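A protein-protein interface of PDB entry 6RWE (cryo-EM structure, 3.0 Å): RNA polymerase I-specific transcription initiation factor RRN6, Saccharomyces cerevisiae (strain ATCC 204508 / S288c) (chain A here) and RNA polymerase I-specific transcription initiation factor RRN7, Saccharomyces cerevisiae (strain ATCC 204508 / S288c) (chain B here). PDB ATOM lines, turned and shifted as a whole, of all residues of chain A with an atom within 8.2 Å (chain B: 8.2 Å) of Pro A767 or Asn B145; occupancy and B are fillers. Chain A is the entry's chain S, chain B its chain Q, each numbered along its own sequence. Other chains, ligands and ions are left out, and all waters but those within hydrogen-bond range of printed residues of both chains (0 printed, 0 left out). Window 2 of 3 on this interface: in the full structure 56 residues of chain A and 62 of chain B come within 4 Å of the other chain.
The backbone carbonyl oxygen (O) of Lys B139 sits at hydrogen-bond distance from the side-chain hydroxyl (OG1) of Thr B143, at 3.3 Å.
ND2 of Asn B145 sits at hydrogen-bond distance from O of Ser A765, 3.2 Å away.
Printed residues of chain B that touch a printed residue of chain A: Leu B105, Leu B138, Lys B139, Lys B142 and Asn B145. Of the 13 printed residues of chain A, 6 touch a printed residue of chain B. Hydrophobic or aromatic side chains of chain A that line the printed part of chain B: Pro A767. Among the printed residues, no Asp or Glu carboxylate lies within 4 Å of a Lys or Arg side-chain nitrogen of the other chain.
Printed residues of chain B within 4 Å of Ser A765: Lys B142 and Asn B145. Pro A767 touches just one residue of chain B: Asn B145. Of the printed residues of chain B, Ser A773 touches Leu B105 (3.5 Å). Of the printed residues of chain A, Lys B139 touches Arg A762. Of chain A, only Ser A765, Gly A766 and Pro A767 come within 4 Å of Asn B145. The nearest residue of chain B that does not touch Pro A767 is Gln B149 (6.9 Å).
Among the printed residues, pairs that only touch across the chains: Ser A774 with Leu B138 (3.3 Å), Pro A767 with Asn B145 (3.3 Å), Gly A766 with Asn B145 (3.4 Å), Arg A762 with Lys B139 (3.4 Å), Ser A773 with Leu B105 (3.5 Å), Arg A762 with Leu B138 (3.7 Å) and Ser A765 with Lys B142 (3.9 Å).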
ATOM      1  N   ARG A 762     -22.899  18.559 -23.596  1.00  0.00           N
ATOM      2  CA  ARG A 762     -21.841  18.738 -24.577  1.00  0.00           C
ATOM      3  C   ARG A 762     -20.883  19.845 -24.159  1.00  0.00           C
ATOM      4  O   ARG A 762     -19.678  19.749 -24.418  1.00  0.00           O
ATOM      5  CB  ARG A 762     -22.456  19.023 -25.947  1.00  0.00           C
ATOM      6  CG  ARG A 762     -21.455  19.218 -27.064  1.00  0.00           C
ATOM      7  CD  ARG A 762     -20.634  17.962 -27.300  1.00  0.00           C
ATOM      8  NE  ARG A 762     -21.456  16.858 -27.779  1.00  0.00           N
ATOM      9  CZ  ARG A 762     -21.033  15.602 -27.865  1.00  0.00           C
ATOM     10  NH1 ARG A 762     -21.848  14.655 -28.310  1.00  0.00           N
ATOM     11  NH2 ARG A 762     -19.794  15.298 -27.508  1.00  0.00           N
ATOM     12  N   SER A 763     -21.390  20.879 -23.481  1.00  0.00           N
ATOM     13  CA  SER A 763     -20.517  21.905 -22.922  1.00  0.00           C
ATOM     14  C   SER A 763     -19.671  21.379 -21.773  1.00  0.00           C
ATOM     15  O   SER A 763     -18.613  21.949 -21.489  1.00  0.00           O
ATOM     16  CB  SER A 763     -21.336  23.105 -22.448  1.00  0.00           C
ATOM     17  OG  SER A 763     -20.501  24.078 -21.843  1.00  0.00           O
ATOM     18  N   LEU A 764     -20.119  20.316 -21.101  1.00  0.00           N
ATOM     19  CA  LEU A 764     -19.257  19.623 -20.153  1.00  0.00           C
ATOM     20  C   LEU A 764     -18.103  18.923 -20.858  1.00  0.00           C
ATOM     21  O   LEU A 764     -17.007  18.822 -20.298  1.00  0.00           O
ATOM     22  CB  LEU A 764     -20.069  18.614 -19.342  1.00  0.00           C
ATOM     23  CG  LEU A 764     -21.053  19.168 -18.310  1.00  0.00           C
ATOM     24  CD1 LEU A 764     -21.951  18.065 -17.775  1.00  0.00           C
ATOM     25  CD2 LEU A 764     -20.298  19.842 -17.176  1.00  0.00           C
ATOM     26  N   SER A 765     -18.322  18.455 -22.090  1.00  0.00           N
ATOM     27  CA  SER A 765     -17.279  17.748 -22.824  1.00  0.00           C
ATOM     28  C   SER A 765     -16.187  18.679 -23.334  1.00  0.00           C
ATOM     29  O   SER A 765     -15.159  18.198 -23.821  1.00  0.00           O
ATOM     30  CB  SER A 765     -17.890  16.973 -23.991  1.00  0.00           C
ATOM     31  OG  SER A 765     -16.893  16.275 -24.713  1.00  0.00           O
ATOM     32  N   GLY A 766     -16.391  19.992 -23.260  1.00  0.00           N
ATOM     33  CA  GLY A 766     -15.345  20.946 -23.532  1.00  0.00           C
ATOM     34  C   GLY A 766     -14.767  21.498 -22.246  1.00  0.00           C
ATOM     35  O   GLY A 766     -15.417  21.479 -21.195  1.00  0.00           O
ATOM     36  N   PRO A 767     -13.542  22.008 -22.297  1.00  0.00           N
ATOM     37  CA  PRO A 767     -12.894  22.539 -21.094  1.00  0.00           C
ATOM     38  C   PRO A 767     -13.441  23.918 -20.737  1.00  0.00           C
ATOM     39  O   PRO A 767     -14.371  24.431 -21.355  1.00  0.00           O
ATOM     40  CB  PRO A 767     -11.421  22.619 -21.500  1.00  0.00           C
ATOM     41  CG  PRO A 767     -11.458  22.827 -22.966  1.00  0.00           C
ATOM     42  CD  PRO A 767     -12.642  22.048 -23.463  1.00  0.00           C
ATOM     43  N   TYR A 768     -12.828  24.523 -19.717  1.00  0.00           N
ATOM     44  CA  TYR A 768     -13.118  25.913 -19.391  1.00  0.00           C
ATOM     45  C   TYR A 768     -12.357  26.888 -20.281  1.00  0.00           C
ATOM     46  O   TYR A 768     -12.503  28.103 -20.113  1.00  0.00           O
ATOM     47  CB  TYR A 768     -12.834  26.196 -17.907  1.00  0.00           C
ATOM     48  CG  TYR A 768     -11.391  26.062 -17.466  1.00  0.00           C
ATOM     49  CD1 TYR A 768     -10.884  24.836 -17.049  1.00  0.00           C
ATOM     50  CD2 TYR A 768     -10.548  27.169 -17.426  1.00  0.00           C
ATOM     51  CE1 TYR A 768      -9.568  24.710 -16.633  1.00  0.00           C
ATOM     52  CE2 TYR A 768      -9.230  27.053 -17.013  1.00  0.00           C
ATOM     53  CZ  TYR A 768      -8.748  25.822 -16.617  1.00  0.00           C
ATOM     54  OH  TYR A 768      -7.443  25.706 -16.202  1.00  0.00           O
ATOM     55  N   GLN A 769     -11.545  26.379 -21.209  1.00  0.00           N
ATOM     56  CA  GLN A 769     -11.008  27.212 -22.277  1.00  0.00           C
ATOM     57  C   GLN A 769     -12.119  27.706 -23.200  1.00  0.00           C
ATOM     58  O   GLN A 769     -12.080  28.846 -23.675  1.00  0.00           O
ATOM     59  CB  GLN A 769      -9.964  26.420 -23.064  1.00  0.00           C
ATOM     60  CG  GLN A 769      -9.291  27.189 -24.175  1.00  0.00           C
ATOM     61  CD  GLN A 769      -8.487  28.353 -23.657  1.00  0.00           C
ATOM     62  OE1 GLN A 769      -8.917  29.501 -23.732  1.00  0.00           O
ATOM     63  NE2 GLN A 769      -7.305  28.066 -23.131  1.00  0.00           N
ATOM     64  N   ASP A 770     -13.127  26.868 -23.451  1.00  0.00           N
ATOM     65  CA  ASP A 770     -14.142  27.148 -24.459  1.00  0.00           C
ATOM     66  C   ASP A 770     -15.512  27.440 -23.859  1.00  0.00           C
ATOM     67  O   ASP A 770     -16.516  27.384 -24.577  1.00  0.00           O
ATOM     68  CB  ASP A 770     -14.256  25.978 -25.433  1.00  0.00           C
ATOM     69  CG  ASP A 770     -12.972  25.705 -26.156  1.00  0.00           C
ATOM     70  OD1 ASP A 770     -12.140  26.623 -26.236  1.00  0.00           O
ATOM     71  OD2 ASP A 770     -12.801  24.580 -26.663  1.00  0.00           O
ATOM     72  N   ILE A 771     -15.588  27.727 -22.560  1.00  0.00           N
ATOM     73  CA  ILE A 771     -16.882  28.071 -21.975  1.00  0.00           C
ATOM     74  C   ILE A 771     -17.303  29.470 -22.404  1.00  0.00           C
ATOM     75  O   ILE A 771     -18.457  29.694 -22.793  1.00  0.00           O
ATOM     76  CB  ILE A 771     -16.837  27.922 -20.442  1.00  0.00           C
ATOM     77  CG1 ILE A 771     -16.670  26.454 -20.055  1.00  0.00           C
ATOM     78  CG2 ILE A 771     -18.088  28.489 -19.786  1.00  0.00           C
ATOM     79  CD1 ILE A 771     -17.806  25.562 -20.502  1.00  0.00           C
ATOM     80  N   ILE A 772     -16.370  30.423 -22.365  1.00  0.00           N
ATOM     81  CA  ILE A 772     -16.668  31.787 -22.788  1.00  0.00           C
ATOM     82  C   ILE A 772     -16.899  31.837 -24.292  1.00  0.00           C
ATOM     83  O   ILE A 772     -17.777  32.566 -24.774  1.00  0.00           O
ATOM     84  CB  ILE A 772     -15.531  32.722 -22.338  1.00  0.00           C
ATOM     85  CG1 ILE A 772     -15.335  32.610 -20.826  1.00  0.00           C
ATOM     86  CG2 ILE A 772     -15.815  34.171 -22.717  1.00  0.00           C
ATOM     87  CD1 ILE A 772     -16.556  32.995 -20.017  1.00  0.00           C
ATOM     88  N   SER A 773     -16.174  31.017 -25.051  1.00  0.00           N
ATOM     89  CA  SER A 773     -16.395  30.888 -26.486  1.00  0.00           C
ATOM     90  C   SER A 773     -17.660  30.117 -26.834  1.00  0.00           C
ATOM     91  O   SER A 773     -17.982  30.018 -28.020  1.00  0.00           O
ATOM     92  CB  SER A 773     -15.195  30.207 -27.138  1.00  0.00           C
ATOM     93  OG  SER A 773     -15.412  30.021 -28.523  1.00  0.00           O
ATOM     94  N   SER A 774     -18.366  29.556 -25.858  1.00  0.00           N
ATOM     95  CA  SER A 774     -19.664  28.922 -26.071  1.00  0.00           C
ATOM     96  C   SER A 774     -20.685  29.675 -25.228  1.00  0.00           C
ATOM     97  O   SER A 774     -21.011  29.263 -24.112  1.00  0.00           O
ATOM     98  CB  SER A 774     -19.628  27.459 -25.708  1.00  0.00           C
ATOM     99  OG  SER A 774     -20.922  26.899 -25.811  1.00  0.00           O
ATOM    100  N   LEU B 105     -13.779  31.953 -33.069  1.00  0.00           N
ATOM    101  CA  LEU B 105     -14.986  31.221 -32.736  1.00  0.00           C
ATOM    102  C   LEU B 105     -16.004  32.082 -32.013  1.00  0.00           C
ATOM    103  O   LEU B 105     -17.204  31.806 -32.104  1.00  0.00           O
ATOM    104  CB  LEU B 105     -14.620  30.014 -31.881  1.00  0.00           C
ATOM    105  CG  LEU B 105     -13.756  29.016 -32.643  1.00  0.00           C
ATOM    106  CD1 LEU B 105     -13.241  27.936 -31.719  1.00  0.00           C
ATOM    107  CD2 LEU B 105     -14.579  28.419 -33.750  1.00  0.00           C
ATOM    108  N   LEU B 138     -22.314  22.929 -31.260  1.00  0.00           N
ATOM    109  CA  LEU B 138     -21.494  22.539 -30.118  1.00  0.00           C
ATOM    110  C   LEU B 138     -20.651  21.306 -30.403  1.00  0.00           C
ATOM    111  O   LEU B 138     -19.512  21.215 -29.931  1.00  0.00           O
ATOM    112  CB  LEU B 138     -22.361  22.305 -28.886  1.00  0.00           C
ATOM    113  CG  LEU B 138     -22.868  23.575 -28.216  1.00  0.00           C
ATOM    114  CD1 LEU B 138     -23.801  23.249 -27.073  1.00  0.00           C
ATOM    115  CD2 LEU B 138     -21.687  24.369 -27.735  1.00  0.00           C
ATOM    116  N   LYS B 139     -21.185  20.348 -31.155  1.00  0.00           N
ATOM    117  CA  LYS B 139     -20.381  19.188 -31.513  1.00  0.00           C
ATOM    118  C   LYS B 139     -19.283  19.535 -32.505  1.00  0.00           C
ATOM    119  O   LYS B 139     -18.248  18.857 -32.519  1.00  0.00           O
ATOM    120  CB  LYS B 139     -21.263  18.079 -32.082  1.00  0.00           C
ATOM    121  CG  LYS B 139     -22.186  17.445 -31.069  1.00  0.00           C
ATOM    122  CD  LYS B 139     -22.822  16.202 -31.642  1.00  0.00           C
ATOM    123  CE  LYS B 139     -23.856  16.555 -32.693  1.00  0.00           C
ATOM    124  NZ  LYS B 139     -24.555  15.348 -33.211  1.00  0.00           N
ATOM    125  N   ILE B 140     -19.517  20.608 -33.264  1.00  0.00           N
ATOM    126  CA  ILE B 140     -18.534  21.214 -34.203  1.00  0.00           C
ATOM    127  C   ILE B 140     -17.351  21.690 -33.353  1.00  0.00           C
ATOM    128  O   ILE B 140     -16.199  21.471 -33.772  1.00  0.00           O
ATOM    129  CB  ILE B 140     -19.166  22.365 -35.012  1.00  0.00           C
ATOM    130  CG1 ILE B 140     -20.194  21.851 -36.024  1.00  0.00           C
ATOM    131  CG2 ILE B 140     -18.090  23.202 -35.684  1.00  0.00           C
ATOM    132  CD1 ILE B 140     -19.583  21.136 -37.206  1.00  0.00           C
ATOM    133  N   LEU B 141     -17.634  22.285 -32.184  1.00  0.00           N
ATOM    134  CA  LEU B 141     -16.608  22.784 -31.279  1.00  0.00           C
ATOM    135  C   LEU B 141     -15.841  21.649 -30.609  1.00  0.00           C
ATOM    136  O   LEU B 141     -14.648  21.799 -30.319  1.00  0.00           O
ATOM    137  CB  LEU B 141     -17.247  23.705 -30.241  1.00  0.00           C
ATOM    138  CG  LEU B 141     -16.320  24.395 -29.240  1.00  0.00           C
ATOM    139  CD1 LEU B 141     -15.301  25.248 -29.970  1.00  0.00           C
ATOM    140  CD2 LEU B 141     -17.115  25.229 -28.254  1.00  0.00           C
ATOM    141  N   LYS B 142     -16.491  20.501 -30.396  1.00  0.00           N
ATOM    142  CA  LYS B 142     -15.794  19.359 -29.810  1.00  0.00           C
ATOM    143  C   LYS B 142     -14.783  18.762 -30.783  1.00  0.00           C
ATOM    144  O   LYS B 142     -13.752  18.234 -30.354  1.00  0.00           O
ATOM    145  CB  LYS B 142     -16.808  18.303 -29.351  1.00  0.00           C
ATOM    146  CG  LYS B 142     -16.220  17.170 -28.497  1.00  0.00           C
ATOM    147  CD  LYS B 142     -15.941  15.899 -29.303  1.00  0.00           C
ATOM    148  CE  LYS B 142     -15.344  14.806 -28.442  1.00  0.00           C
ATOM    149  NZ  LYS B 142     -13.976  15.181 -27.988  1.00  0.00           N
ATOM    150  N   THR B 143     -15.067  18.824 -32.086  1.00  0.00           N
ATOM    151  CA  THR B 143     -14.084  18.410 -33.079  1.00  0.00           C
ATOM    152  C   THR B 143     -12.873  19.332 -33.056  1.00  0.00           C
ATOM    153  O   THR B 143     -11.734  18.879 -33.231  1.00  0.00           O
ATOM    154  CB  THR B 143     -14.737  18.387 -34.461  1.00  0.00           C
ATOM    155  OG1 THR B 143     -15.902  17.557 -34.413  1.00  0.00           O
ATOM    156  CG2 THR B 143     -13.793  17.825 -35.508  1.00  0.00           C
ATOM    157  N   ILE B 144     -13.139  20.609 -32.777  1.00  0.00           N
ATOM    158  CA  ILE B 144     -12.106  21.666 -32.585  1.00  0.00           C
ATOM    159  C   ILE B 144     -11.347  21.327 -31.295  1.00  0.00           C
ATOM    160  O   ILE B 144     -10.111  21.476 -31.280  1.00  0.00           O
ATOM    161  CB  ILE B 144     -12.746  23.067 -32.533  1.00  0.00           C
ATOM    162  CG1 ILE B 144     -13.578  23.354 -33.785  1.00  0.00           C
ATOM    163  CG2 ILE B 144     -11.689  24.135 -32.300  1.00  0.00           C
ATOM    164  CD1 ILE B 144     -12.828  23.141 -35.079  1.00  0.00           C
ATOM    165  N   ASN B 145     -12.069  20.849 -30.271  1.00  0.00           N
ATOM    166  CA  ASN B 145     -11.508  20.511 -28.969  1.00  0.00           C
ATOM    167  C   ASN B 145     -10.582  19.302 -29.049  1.00  0.00           C
ATOM    168  O   ASN B 145      -9.553  19.262 -28.365  1.00  0.00           O
ATOM    169  CB  ASN B 145     -12.647  20.232 -27.992  1.00  0.00           C
ATOM    170  CG  ASN B 145     -12.189  20.135 -26.559  1.00  0.00           C
ATOM    171  OD1 ASN B 145     -11.049  20.458 -26.224  1.00  0.00           O
ATOM    172  ND2 ASN B 145     -13.068  19.628 -25.705  1.00  0.00           N
ATOM    173  N   ASP B 146     -10.930  18.316 -29.879  1.00  0.00           N
ATOM    174  CA  ASP B 146     -10.162  17.078 -29.963  1.00  0.00           C
ATOM    175  C   ASP B 146      -8.789  17.281 -30.581  1.00  0.00           C
ATOM    176  O   ASP B 146      -7.860  16.534 -30.257  1.00  0.00           O
ATOM    177  CB  ASP B 146     -10.940  16.041 -30.773  1.00  0.00           C
ATOM    178  CG  ASP B 146     -10.242  14.698 -30.822  1.00  0.00           C
ATOM    179  OD1 ASP B 146     -10.263  13.976 -29.802  1.00  0.00           O
ATOM    180  OD2 ASP B 146      -9.658  14.375 -31.879  1.00  0.00           O
ATOM    181  N   GLN B 147      -8.642  18.277 -31.444  1.00  0.00           N
ATOM    182  CA  GLN B 147      -7.373  18.516 -32.100  1.00  0.00           C
ATOM    183  C   GLN B 147      -6.349  19.052 -31.101  1.00  0.00           C
ATOM    184  O   GLN B 147      -6.706  19.771 -30.162  1.00  0.00           O
ATOM    185  CB  GLN B 147      -7.555  19.502 -33.247  1.00  0.00           C
ATOM    186  CG  GLN B 147      -8.401  18.956 -34.379  1.00  0.00           C
ATOM    187  CD  GLN B 147      -8.645  19.985 -35.454  1.00  0.00           C
ATOM    188  OE1 GLN B 147      -8.256  21.143 -35.317  1.00  0.00           O
ATOM    189  NE2 GLN B 147      -9.292  19.570 -36.534  1.00  0.00           N
ATOM    190  N   PRO B 148      -5.069  18.678 -31.259  1.00  0.00           N
ATOM    191  CA  PRO B 148      -3.993  19.239 -30.414  1.00  0.00           C
ATOM    192  C   PRO B 148      -3.861  20.740 -30.631  1.00  0.00           C
ATOM    193  O   PRO B 148      -3.630  21.213 -31.749  1.00  0.00           O
ATOM    194  CB  PRO B 148      -2.760  18.457 -30.884  1.00  0.00           C
ATOM    195  CG  PRO B 148      -3.298  17.213 -31.495  1.00  0.00           C
ATOM    196  CD  PRO B 148      -4.571  17.615 -32.149  1.00  0.00           C
ATOM    197  N   GLN B 149      -4.056  21.485 -29.538  1.00  0.00           N
ATOM    198  CA  GLN B 149      -4.166  22.942 -29.518  1.00  0.00           C
ATOM    199  C   GLN B 149      -2.995  23.664 -30.175  1.00  0.00           C
ATOM    200  O   GLN B 149      -3.183  24.712 -30.801  1.00  0.00           O
ATOM    201  CB  GLN B 149      -4.334  23.424 -28.078  1.00  0.00           C
ATOM    202  CG  GLN B 149      -5.628  22.959 -27.456  1.00  0.00           C
ATOM    203  CD  GLN B 149      -6.837  23.483 -28.196  1.00  0.00           C
ATOM    204  OE1 GLN B 149      -7.508  22.743 -28.917  1.00  0.00           O
ATOM    205  NE2 GLN B 149      -7.134  24.762 -28.011  1.00  0.00           N
ATOM    206  N   LEU B 152      -3.515  23.694 -34.518  1.00  0.00           N
ATOM    207  CA  LEU B 152      -4.677  22.832 -34.708  1.00  0.00           C
ATOM    208  C   LEU B 152      -5.301  23.016 -36.087  1.00  0.00           C
ATOM    209  O   LEU B 152      -5.832  22.051 -36.652  1.00  0.00           O
ATOM    210  CB  LEU B 152      -5.706  23.067 -33.598  1.00  0.00           C
ATOM    211  CG  LEU B 152      -6.546  24.338 -33.471  1.00  0.00           C
ATOM    212  CD1 LEU B 152      -7.738  24.035 -32.602  1.00  0.00           C
ATOM    213  CD2 LEU B 152      -5.761  25.473 -32.845  1.00  0.00           C
ATOM    214  N   LEU B 154      -8.201  24.586 -37.298  1.00  0.00           N
ATOM    215  CA  LEU B 154      -9.647  24.273 -37.441  1.00  0.00           C
ATOM    216  C   LEU B 154     -10.101  24.807 -38.801  1.00  0.00           C
ATOM    217  O   LEU B 154      -9.779  25.966 -39.104  1.00  0.00           O
ATOM    218  CB  LEU B 154     -10.405  24.995 -36.324  1.00  0.00           C
ATOM    219  CG  LEU B 154     -10.526  26.508 -36.492  1.00  0.00           C
ATOM    220  CD1 LEU B 154     -11.175  27.140 -35.271  1.00  0.00           C
ATOM    221  CD2 LEU B 154      -9.165  27.133 -36.745  1.00  0.00           C
